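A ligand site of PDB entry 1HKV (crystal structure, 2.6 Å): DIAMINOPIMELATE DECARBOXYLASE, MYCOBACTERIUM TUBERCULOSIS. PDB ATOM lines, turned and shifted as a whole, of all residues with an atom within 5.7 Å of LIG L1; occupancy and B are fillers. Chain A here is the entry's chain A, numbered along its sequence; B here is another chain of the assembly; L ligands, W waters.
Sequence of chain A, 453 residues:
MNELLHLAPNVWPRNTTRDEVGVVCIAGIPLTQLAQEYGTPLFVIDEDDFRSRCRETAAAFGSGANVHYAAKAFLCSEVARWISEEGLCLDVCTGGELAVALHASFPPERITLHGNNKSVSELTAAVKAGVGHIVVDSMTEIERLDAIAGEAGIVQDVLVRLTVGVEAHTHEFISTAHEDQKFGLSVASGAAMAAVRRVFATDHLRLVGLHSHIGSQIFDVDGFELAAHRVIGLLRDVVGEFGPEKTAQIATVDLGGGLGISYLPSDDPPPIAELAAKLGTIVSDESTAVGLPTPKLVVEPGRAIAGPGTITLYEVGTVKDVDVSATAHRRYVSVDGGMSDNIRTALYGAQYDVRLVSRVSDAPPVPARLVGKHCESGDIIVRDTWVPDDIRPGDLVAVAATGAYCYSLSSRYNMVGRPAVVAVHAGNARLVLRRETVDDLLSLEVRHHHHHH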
ATOM      1  N   ALA A  70      15.904   5.261 -10.463  1.00  0.00           N
ATOM      2  CA  ALA A  70      16.622   6.307 -11.050  1.00  0.00           C
ATOM      3  C   ALA A  70      16.129   7.595 -10.499  1.00  0.00           C
ATOM      4  O   ALA A  70      15.062   8.080 -10.868  1.00  0.00           O
ATOM      5  CB  ALA A  70      16.401   6.291 -12.549  1.00  0.00           C
ATOM      6  N   LYS A  72      16.689  10.620 -10.910  1.00  0.00           N
ATOM      7  CA  LYS A  72      16.494  11.806 -11.739  1.00  0.00           C
ATOM      8  C   LYS A  72      14.989  11.994 -12.035  1.00  0.00           C
ATOM      9  O   LYS A  72      14.550  13.111 -12.252  1.00  0.00           O
ATOM     10  CB  LYS A  72      17.277  11.670 -13.015  1.00  0.00           C
ATOM     11  CG  LYS A  72      17.028  10.298 -13.738  1.00  0.00           C
ATOM     12  CD  LYS A  72      18.059  10.022 -14.822  1.00  0.00           C
ATOM     13  CE  LYS A  72      17.613  10.501 -16.173  1.00  0.00           C
ATOM     14  NZ  LYS A  72      17.723   9.339 -17.076  1.00  0.00           N
ATOM     15  N   ALA A  73      14.228  10.889 -12.043  1.00  0.00           N
ATOM     16  CA  ALA A  73      12.812  10.979 -12.358  1.00  0.00           C
ATOM     17  C   ALA A  73      12.092  11.916 -11.324  1.00  0.00           C
ATOM     18  O   ALA A  73      11.283  12.763 -11.687  1.00  0.00           O
ATOM     19  CB  ALA A  73      12.200   9.626 -12.395  1.00  0.00           C
ATOM     20  N   ASP A  91      19.845   5.192  -7.843  1.00  0.00           N
ATOM     21  CA  ASP A  91      20.851   5.572  -8.811  1.00  0.00           C
ATOM     22  C   ASP A  91      20.941   7.051  -8.717  1.00  0.00           C
ATOM     23  O   ASP A  91      19.965   7.755  -8.964  1.00  0.00           O
ATOM     24  CB  ASP A  91      20.435   5.206 -10.234  1.00  0.00           C
ATOM     25  CG  ASP A  91      20.852   3.789 -10.675  1.00  0.00           C
ATOM     26  OD1 ASP A  91      21.063   2.884  -9.857  1.00  0.00           O
ATOM     27  OD2 ASP A  91      20.932   3.502 -11.882  1.00  0.00           O
ATOM     28  N   HIS A 114      26.100   7.393 -11.238  1.00  0.00           N
ATOM     29  CA  HIS A 114      26.160   7.473 -12.721  1.00  0.00           C
ATOM     30  C   HIS A 114      26.665   8.835 -13.149  1.00  0.00           C
ATOM     31  O   HIS A 114      26.661   9.818 -12.359  1.00  0.00           O
ATOM     32  CB  HIS A 114      24.766   7.310 -13.289  1.00  0.00           C
ATOM     33  CG  HIS A 114      24.327   5.897 -13.485  1.00  0.00           C
ATOM     34  ND1 HIS A 114      24.836   5.090 -14.481  1.00  0.00           N
ATOM     35  CD2 HIS A 114      23.407   5.157 -12.845  1.00  0.00           C
ATOM     36  CE1 HIS A 114      24.254   3.903 -14.424  1.00  0.00           C
ATOM     37  NE2 HIS A 114      23.376   3.921 -13.438  1.00  0.00           N
ATOM     38  N   ARG A 161      30.033   1.407 -18.599  1.00  0.00           N
ATOM     39  CA  ARG A 161      28.873   1.754 -19.361  1.00  0.00           C
ATOM     40  C   ARG A 161      29.194   1.526 -20.803  1.00  0.00           C
ATOM     41  O   ARG A 161      30.204   1.995 -21.273  1.00  0.00           O
ATOM     42  CB  ARG A 161      28.462   3.214 -19.114  1.00  0.00           C
ATOM     43  CG  ARG A 161      27.199   3.692 -19.942  1.00  0.00           C
ATOM     44  CD  ARG A 161      26.421   4.751 -19.296  1.00  0.00           C
ATOM     45  NE  ARG A 161      25.191   5.069 -19.989  1.00  0.00           N
ATOM     46  CZ  ARG A 161      24.323   5.961 -19.557  1.00  0.00           C
ATOM     47  NH1 ARG A 161      24.529   6.582 -18.435  1.00  0.00           N
ATOM     48  NH2 ARG A 161      23.236   6.232 -20.236  1.00  0.00           N
ATOM     49  N   PHE A 183      27.482   9.297 -23.689  1.00  0.00           N
ATOM     50  CA  PHE A 183      27.625   8.261 -22.694  1.00  0.00           C
ATOM     51  C   PHE A 183      28.361   7.063 -23.254  1.00  0.00           C
ATOM     52  O   PHE A 183      28.266   6.733 -24.477  1.00  0.00           O
ATOM     53  CB  PHE A 183      26.234   7.763 -22.150  1.00  0.00           C
ATOM     54  CG  PHE A 183      25.595   8.712 -21.204  1.00  0.00           C
ATOM     55  CD1 PHE A 183      26.054   8.842 -19.907  1.00  0.00           C
ATOM     56  CD2 PHE A 183      24.508   9.514 -21.604  1.00  0.00           C
ATOM     57  CE1 PHE A 183      25.458   9.755 -19.008  1.00  0.00           C
ATOM     58  CE2 PHE A 183      23.950  10.403 -20.755  1.00  0.00           C
ATOM     59  CZ  PHE A 183      24.427  10.518 -19.425  1.00  0.00           C
ATOM     60  N   HIS A 211      27.072  -2.211 -18.088  1.00  0.00           N
ATOM     61  CA  HIS A 211      25.862  -1.440 -18.065  1.00  0.00           C
ATOM     62  C   HIS A 211      25.560  -0.959 -19.452  1.00  0.00           C
ATOM     63  O   HIS A 211      26.474  -0.546 -20.205  1.00  0.00           O
ATOM     64  CB  HIS A 211      25.947  -0.249 -17.053  1.00  0.00           C
ATOM     65  CG  HIS A 211      24.867   0.773 -17.217  1.00  0.00           C
ATOM     66  ND1 HIS A 211      24.970   1.834 -18.094  1.00  0.00           N
ATOM     67  CD2 HIS A 211      23.647   0.875 -16.646  1.00  0.00           C
ATOM     68  CE1 HIS A 211      23.880   2.556 -18.036  1.00  0.00           C
ATOM     69  NE2 HIS A 211      23.057   1.989 -17.171  1.00  0.00           N
ATOM     70  N   HIS A 213      22.220   1.527 -21.256  1.00  0.00           N
ATOM     71  CA  HIS A 213      20.927   2.213 -21.214  1.00  0.00           C
ATOM     72  C   HIS A 213      20.543   2.644 -22.591  1.00  0.00           C
ATOM     73  O   HIS A 213      21.258   3.406 -23.197  1.00  0.00           O
ATOM     74  CB  HIS A 213      20.992   3.449 -20.292  1.00  0.00           C
ATOM     75  CG  HIS A 213      19.676   4.192 -20.180  1.00  0.00           C
ATOM     76  ND1 HIS A 213      18.537   3.587 -19.672  1.00  0.00           N
ATOM     77  CD2 HIS A 213      19.333   5.467 -20.512  1.00  0.00           C
ATOM     78  CE1 HIS A 213      17.552   4.469 -19.676  1.00  0.00           C
ATOM     79  NE2 HIS A 213      18.009   5.608 -20.180  1.00  0.00           N
ATOM     80  N   GLY A 215      17.109   3.734 -24.000  1.00  0.00           N
ATOM     81  CA  GLY A 215      15.991   4.591 -24.384  1.00  0.00           C
ATOM     82  C   GLY A 215      14.983   4.982 -23.305  1.00  0.00           C
ATOM     83  O   GLY A 215      15.244   4.970 -22.133  1.00  0.00           O
ATOM     84  N   SER A 216      13.831   5.411 -23.741  1.00  0.00           N
ATOM     85  CA  SER A 216      12.776   5.655 -22.832  1.00  0.00           C
ATOM     86  C   SER A 216      11.445   5.349 -23.467  1.00  0.00           C
ATOM     87  O   SER A 216      11.357   5.290 -24.638  1.00  0.00           O
ATOM     88  CB  SER A 216      12.831   7.049 -22.403  1.00  0.00           C
ATOM     89  OG  SER A 216      12.457   7.819 -23.483  1.00  0.00           O
ATOM     90  N   GLN A 217      10.422   5.140 -22.644  1.00  0.00           N
ATOM     91  CA  GLN A 217       9.051   4.874 -23.082  1.00  0.00           C
ATOM     92  C   GLN A 217       8.979   3.637 -23.997  1.00  0.00           C
ATOM     93  O   GLN A 217       8.182   3.550 -24.888  1.00  0.00           O
ATOM     94  CB  GLN A 217       8.439   6.131 -23.761  1.00  0.00           C
ATOM     95  CG  GLN A 217       7.620   7.042 -22.778  1.00  0.00           C
ATOM     96  CD  GLN A 217       6.494   6.244 -22.027  1.00  0.00           C
ATOM     97  OE1 GLN A 217       6.757   5.605 -21.008  1.00  0.00           O
ATOM     98  NE2 GLN A 217       5.284   6.301 -22.536  1.00  0.00           N
ATOM     99  N   GLY A 256      19.865  -1.098 -17.922  1.00  0.00           N
ATOM    100  CA  GLY A 256      19.338   0.267 -17.765  1.00  0.00           C
ATOM    101  C   GLY A 256      17.848   0.407 -17.450  1.00  0.00           C
ATOM    102  O   GLY A 256      17.168  -0.484 -16.996  1.00  0.00           O
ATOM    103  N   GLY A 257      17.356   1.590 -17.700  1.00  0.00           N
ATOM    104  CA  GLY A 257      15.955   1.858 -17.599  1.00  0.00           C
ATOM    105  C   GLY A 257      15.248   1.992 -18.942  1.00  0.00           C
ATOM    106  O   GLY A 257      15.651   1.335 -19.932  1.00  0.00           O
ATOM    107  N   GLY A 258      14.186   2.820 -18.960  1.00  0.00           N
ATOM    108  CA  GLY A 258      13.387   3.090 -20.137  1.00  0.00           C
ATOM    109  C   GLY A 258      12.107   2.271 -20.243  1.00  0.00           C
ATOM    110  O   GLY A 258      11.379   2.349 -21.218  1.00  0.00           O
ATOM    111  N   LEU A 259      11.828   1.493 -19.232  1.00  0.00           N
ATOM    112  CA  LEU A 259      10.558   0.814 -19.120  1.00  0.00           C
ATOM    113  C   LEU A 259       9.434   1.752 -19.075  1.00  0.00           C
ATOM    114  O   LEU A 259       9.420   2.880 -18.544  1.00  0.00           O
ATOM    115  CB  LEU A 259      10.571  -0.344 -18.321  1.00  0.00           C
ATOM    116  CG  LEU A 259      11.827  -0.552 -17.457  1.00  0.00           C
ATOM    117  CD1 LEU A 259      11.550  -1.563 -16.365  1.00  0.00           C
ATOM    118  CD2 LEU A 259      12.980  -1.018 -18.344  1.00  0.00           C
ATOM    119  N   GLU A 300      17.073  -0.376 -14.135  1.00  0.00           N
ATOM    120  CA  GLU A 300      17.148   0.889 -13.494  1.00  0.00           C
ATOM    121  C   GLU A 300      15.940   1.791 -13.733  1.00  0.00           C
ATOM    122  O   GLU A 300      16.100   2.924 -14.158  1.00  0.00           O
ATOM    123  CB  GLU A 300      18.427   1.605 -13.942  1.00  0.00           C
ATOM    124  CG  GLU A 300      19.692   0.887 -13.490  1.00  0.00           C
ATOM    125  CD  GLU A 300      20.939   1.431 -14.109  1.00  0.00           C
ATOM    126  OE1 GLU A 300      22.045   1.023 -13.675  1.00  0.00           O
ATOM    127  OE2 GLU A 300      20.806   2.266 -15.027  1.00  0.00           O
ATOM    128  N   PRO A 301      14.741   1.330 -13.420  1.00  0.00           N
ATOM    129  CA  PRO A 301      13.526   2.097 -13.668  1.00  0.00           C
ATOM    130  C   PRO A 301      13.474   3.446 -13.006  1.00  0.00           C
ATOM    131  O   PRO A 301      13.836   3.573 -11.827  1.00  0.00           O
ATOM    132  CB  PRO A 301      12.414   1.204 -13.089  1.00  0.00           C
ATOM    133  CG  PRO A 301      13.075   0.338 -12.196  1.00  0.00           C
ATOM    134  CD  PRO A 301      14.432   0.061 -12.787  1.00  0.00           C
ATOM    135  N   GLY A 302      13.052   4.441 -13.731  1.00  0.00           N
ATOM    136  CA  GLY A 302      12.780   5.715 -13.151  1.00  0.00           C
ATOM    137  C   GLY A 302      11.298   6.022 -13.175  1.00  0.00           C
ATOM    138  O   GLY A 302      10.586   6.005 -12.162  1.00  0.00           O
ATOM    139  N   ARG A 303      10.861   6.297 -14.376  1.00  0.00           N
ATOM    140  CA  ARG A 303       9.536   6.654 -14.711  1.00  0.00           C
ATOM    141  C   ARG A 303       8.521   5.620 -14.352  1.00  0.00           C
ATOM    142  O   ARG A 303       7.435   5.960 -13.964  1.00  0.00           O
ATOM    143  CB  ARG A 303       9.500   6.861 -16.224  1.00  0.00           C
ATOM    144  CG  ARG A 303       8.182   7.233 -16.830  1.00  0.00           C
ATOM    145  CD  ARG A 303       8.245   7.267 -18.402  1.00  0.00           C
ATOM    146  NE  ARG A 303       8.752   8.541 -18.956  1.00  0.00           N
ATOM    147  CZ  ARG A 303       9.975   8.747 -19.358  1.00  0.00           C
ATOM    148  NH1 ARG A 303      10.313   9.905 -19.841  1.00  0.00           N
ATOM    149  NH2 ARG A 303      10.864   7.819 -19.286  1.00  0.00           N
ATOM    150  N   ALA A 304       8.860   4.328 -14.510  1.00  0.00           N
ATOM    151  CA  ALA A 304       7.849   3.260 -14.400  1.00  0.00           C
ATOM    152  C   ALA A 304       7.531   2.988 -12.949  1.00  0.00           C
ATOM    153  O   ALA A 304       6.671   2.183 -12.633  1.00  0.00           O
ATOM    154  CB  ALA A 304       8.307   2.088 -15.019  1.00  0.00           C
ATOM    155  N   TYR A 405       9.794  13.270 -14.015  1.00  0.00           N
ATOM    156  CA  TYR A 405      10.467  14.222 -14.867  1.00  0.00           C
ATOM    157  C   TYR A 405       9.867  15.589 -14.862  1.00  0.00           C
ATOM    158  O   TYR A 405      10.564  16.551 -15.188  1.00  0.00           O
ATOM    159  CB  TYR A 405      10.737  13.651 -16.313  1.00  0.00           C
ATOM    160  CG  TYR A 405      11.726  12.478 -16.248  1.00  0.00           C
ATOM    161  CD1 TYR A 405      13.080  12.673 -15.939  1.00  0.00           C
ATOM    162  CD2 TYR A 405      11.278  11.186 -16.382  1.00  0.00           C
ATOM    163  CE1 TYR A 405      13.980  11.549 -15.774  1.00  0.00           C
ATOM    164  CE2 TYR A 405      12.155  10.092 -16.223  1.00  0.00           C
ATOM    165  CZ  TYR A 405      13.482  10.297 -15.927  1.00  0.00           C
ATOM    166  OH  TYR A 405      14.260   9.248 -15.841  1.00  0.00           O
ATOM    167  N   CYS B 375      22.262  13.167 -16.449  1.00  0.00           N
ATOM    168  CA  CYS B 375      22.097  11.800 -16.920  1.00  0.00           C
ATOM    169  C   CYS B 375      21.043  11.677 -18.015  1.00  0.00           C
ATOM    170  O   CYS B 375      20.130  10.871 -17.919  1.00  0.00           O
ATOM    171  CB  CYS B 375      21.748  10.858 -15.794  1.00  0.00           C
ATOM    172  SG  CYS B 375      23.155  10.438 -14.879  1.00  0.00           S
ATOM    173  N   GLU B 376      21.235  12.421 -19.095  1.00  0.00           N
ATOM    174  CA  GLU B 376      20.342  12.411 -20.182  1.00  0.00           C
ATOM    175  C   GLU B 376      21.102  12.713 -21.495  1.00  0.00           C
ATOM    176  O   GLU B 376      21.830  13.701 -21.565  1.00  0.00           O
ATOM    177  CB  GLU B 376      19.277  13.477 -19.914  1.00  0.00           C
ATOM    178  CG  GLU B 376      18.097  13.468 -20.882  1.00  0.00           C
ATOM    179  CD  GLU B 376      17.019  14.426 -20.478  1.00  0.00           C
ATOM    180  OE1 GLU B 376      16.415  14.193 -19.403  1.00  0.00           O
ATOM    181  OE2 GLU B 376      16.783  15.415 -21.211  1.00  0.00           O
HETATM  182  N1  LIG L   1      19.459   4.455 -16.113  1.00  0.00           N
HETATM  183  C1  LIG L   1      20.174   5.547 -16.641  1.00  0.00           C
HETATM  184  C2  LIG L   1      21.658   5.439 -16.856  1.00  0.00           C
HETATM  185  C3  LIG L   1      19.528   6.720 -16.955  1.00  0.00           C
HETATM  186  O1  LIG L   1      20.275   7.762 -17.453  1.00  0.00           O
HETATM  187  C4  LIG L   1      18.156   6.850 -16.719  1.00  0.00           C
HETATM  188  C5  LIG L   1      17.503   8.054 -17.024  1.00  0.00           C
HETATM  189  C6  LIG L   1      17.430   5.771 -16.187  1.00  0.00           C
HETATM  190  C7  LIG L   1      18.091   4.563 -15.876  1.00  0.00           C
HETATM  191  C8  LIG L   1      15.913   5.862 -15.964  1.00  0.00           C
HETATM  192  O2  LIG L   1      15.136   6.161 -17.116  1.00  0.00           O
HETATM  193  P1  LIG L   1      13.529   5.949 -17.183  1.00  0.00           P
HETATM  194  O3  LIG L   1      13.146   6.083 -18.605  1.00  0.00           O
HETATM  195  O4  LIG L   1      12.865   7.104 -16.446  1.00  0.00           O
HETATM  196  O5  LIG L   1      13.058   4.546 -16.751  1.00  0.00           O
HETATM  197  N1  LG2 L   2      12.791  11.392 -25.015  1.00  0.00           N
HETATM  198  C1  LG2 L   2      12.427  10.842 -23.703  1.00  0.00           C
HETATM  199  C2  LG2 L   2      10.899  10.810 -23.491  1.00  0.00           C
HETATM  200  O1  LG2 L   2      10.184  10.039 -24.162  1.00  0.00           O
HETATM  201  C3  LG2 L   2      13.152  11.626 -22.535  1.00  0.00           C
HETATM  202  C4  LG2 L   2      14.331  10.830 -21.860  1.00  0.00           C
HETATM  203  C5  LG2 L   2      14.546  11.196 -20.373  1.00  0.00           C
HETATM  204  C6  LG2 L   2      16.009  10.759 -19.825  1.00  0.00           C
HETATM  205  N2  LG2 L   2      16.908   9.881 -20.764  1.00  0.00           N
HETATM  206  O2  LG2 L   2      10.341  11.533 -22.629  1.00  0.00           O
HETATM  207  O   HOH W   1      10.744   4.978 -19.603  1.00  0.00           O
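Water W1 lies within hydrogen-bond range of O of Leu 259 (2.7 Å), O3 of LIG L1 (2.8 Å), NH2 of Arg 303 (2.9 Å), N of Gln 217 (3.1 Å) and O of Gly 258 (3.2 Å).
Ala 70 touches LIG L1 (CB to C8, 3.5 Å). His 114 touches LIG L1. Arg 161 touches LIG L1 (NH1 to C2, 3.5 Å). NE2 of His 211 touches C2 of LIG L1 (3.7 Å). NE2 of His 213 touches C4 of LIG L1 (3.7 Å). CB of Ser 216 touches O3 of LIG L1 (3.9 Å). Gly 257 touches LIG L1. Pro 301 touches LIG L1. Hydrophobic or aromatic side chains within 4 Å of LIG L1: Ala 70, His 114, His 211, His 213 and Tyr 405. 15 residues have an atom within 4 Å of LIG L1: Ala 70, Lys 72, His 114, Arg 161, His 211, His 213, Ser 216, Gly 257, Gly 258, Glu 300, Pro 301, Gly 302, Arg 303, Tyr 405 and Cys 375 of chain B. Along chain A the residues within 4 Å of LIG L1 span positions 70 to 405. The nearest printed residue that does not touch LIG L1 is Leu 259 (4.1 Å).
The guanidinium group of Arg 303 is in salt-bridge range of an oxygen (O2) of LG2 L2, 3.2 Å away. The side-chain carboxylate (OE2) of Glu 300 is in hydrogen-bond range of a nitrogen (N1) of LIG L1 (2.8 Å). O4 of LIG L1 sits at hydrogen-bond distance from N of Arg 303. The backbone NH of Gly 258 sits at hydrogen-bond distance from an oxygen (O5) of LIG L1, 3.0 Å away. O of Cys 375 of chain B lies within hydrogen-bond range of O1 of LIG L1 (3.1 Å). O4 of LIG L1 lies within hydrogen-bond range of OH of Tyr 405, 2.6 Å away. The side-chain hydroxyl of Ser 216 sits close to an oxygen (O1) of LG2 L2, at 3.2 Å. The side-chain amino group (NZ) of Lys 72 is covalently linked to a carbon (C5) of LIG L1 (1.3 Å). An oxygen (O3) of LIG L1 is in salt-bridge range of the guanidinium group (NH2) of Arg 303 (2.9 Å). An oxygen (O5) of LIG L1 is in hydrogen-bond range of the backbone NH (N) of Gly 302 (3.0 Å).
NE2 of His 211 lies within hydrogen-bond range of OE2 of Glu 300 (3.1 Å). N of Tyr 405 lies within hydrogen-bond range of O of Ala 73, 2.8 Å away. The backbone carbonyl oxygen (O) of Gly 215 lies close to a ring nitrogen (NE2) of His 213, 3.4 Å away. The side-chain amino group (NZ) of Lys 72 is in hydrogen-bond range of the backbone carbonyl oxygen (O) of Cys 375 of chain B, 3.0 Å away. O of Pro 301 sits at hydrogen-bond distance from N of Ala 70. A ring nitrogen (ND1) of His 213 lies within hydrogen-bond range of the backbone NH (N) of Gly 257. The backbone NH (N) of Gln 217 sits at hydrogen-bond distance from the backbone carbonyl oxygen (O) of Gly 258. The side-chain carboxylate of Glu 300 is in hydrogen-bond range of a ring nitrogen (NE2) of His 114, at 3.2 Å.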
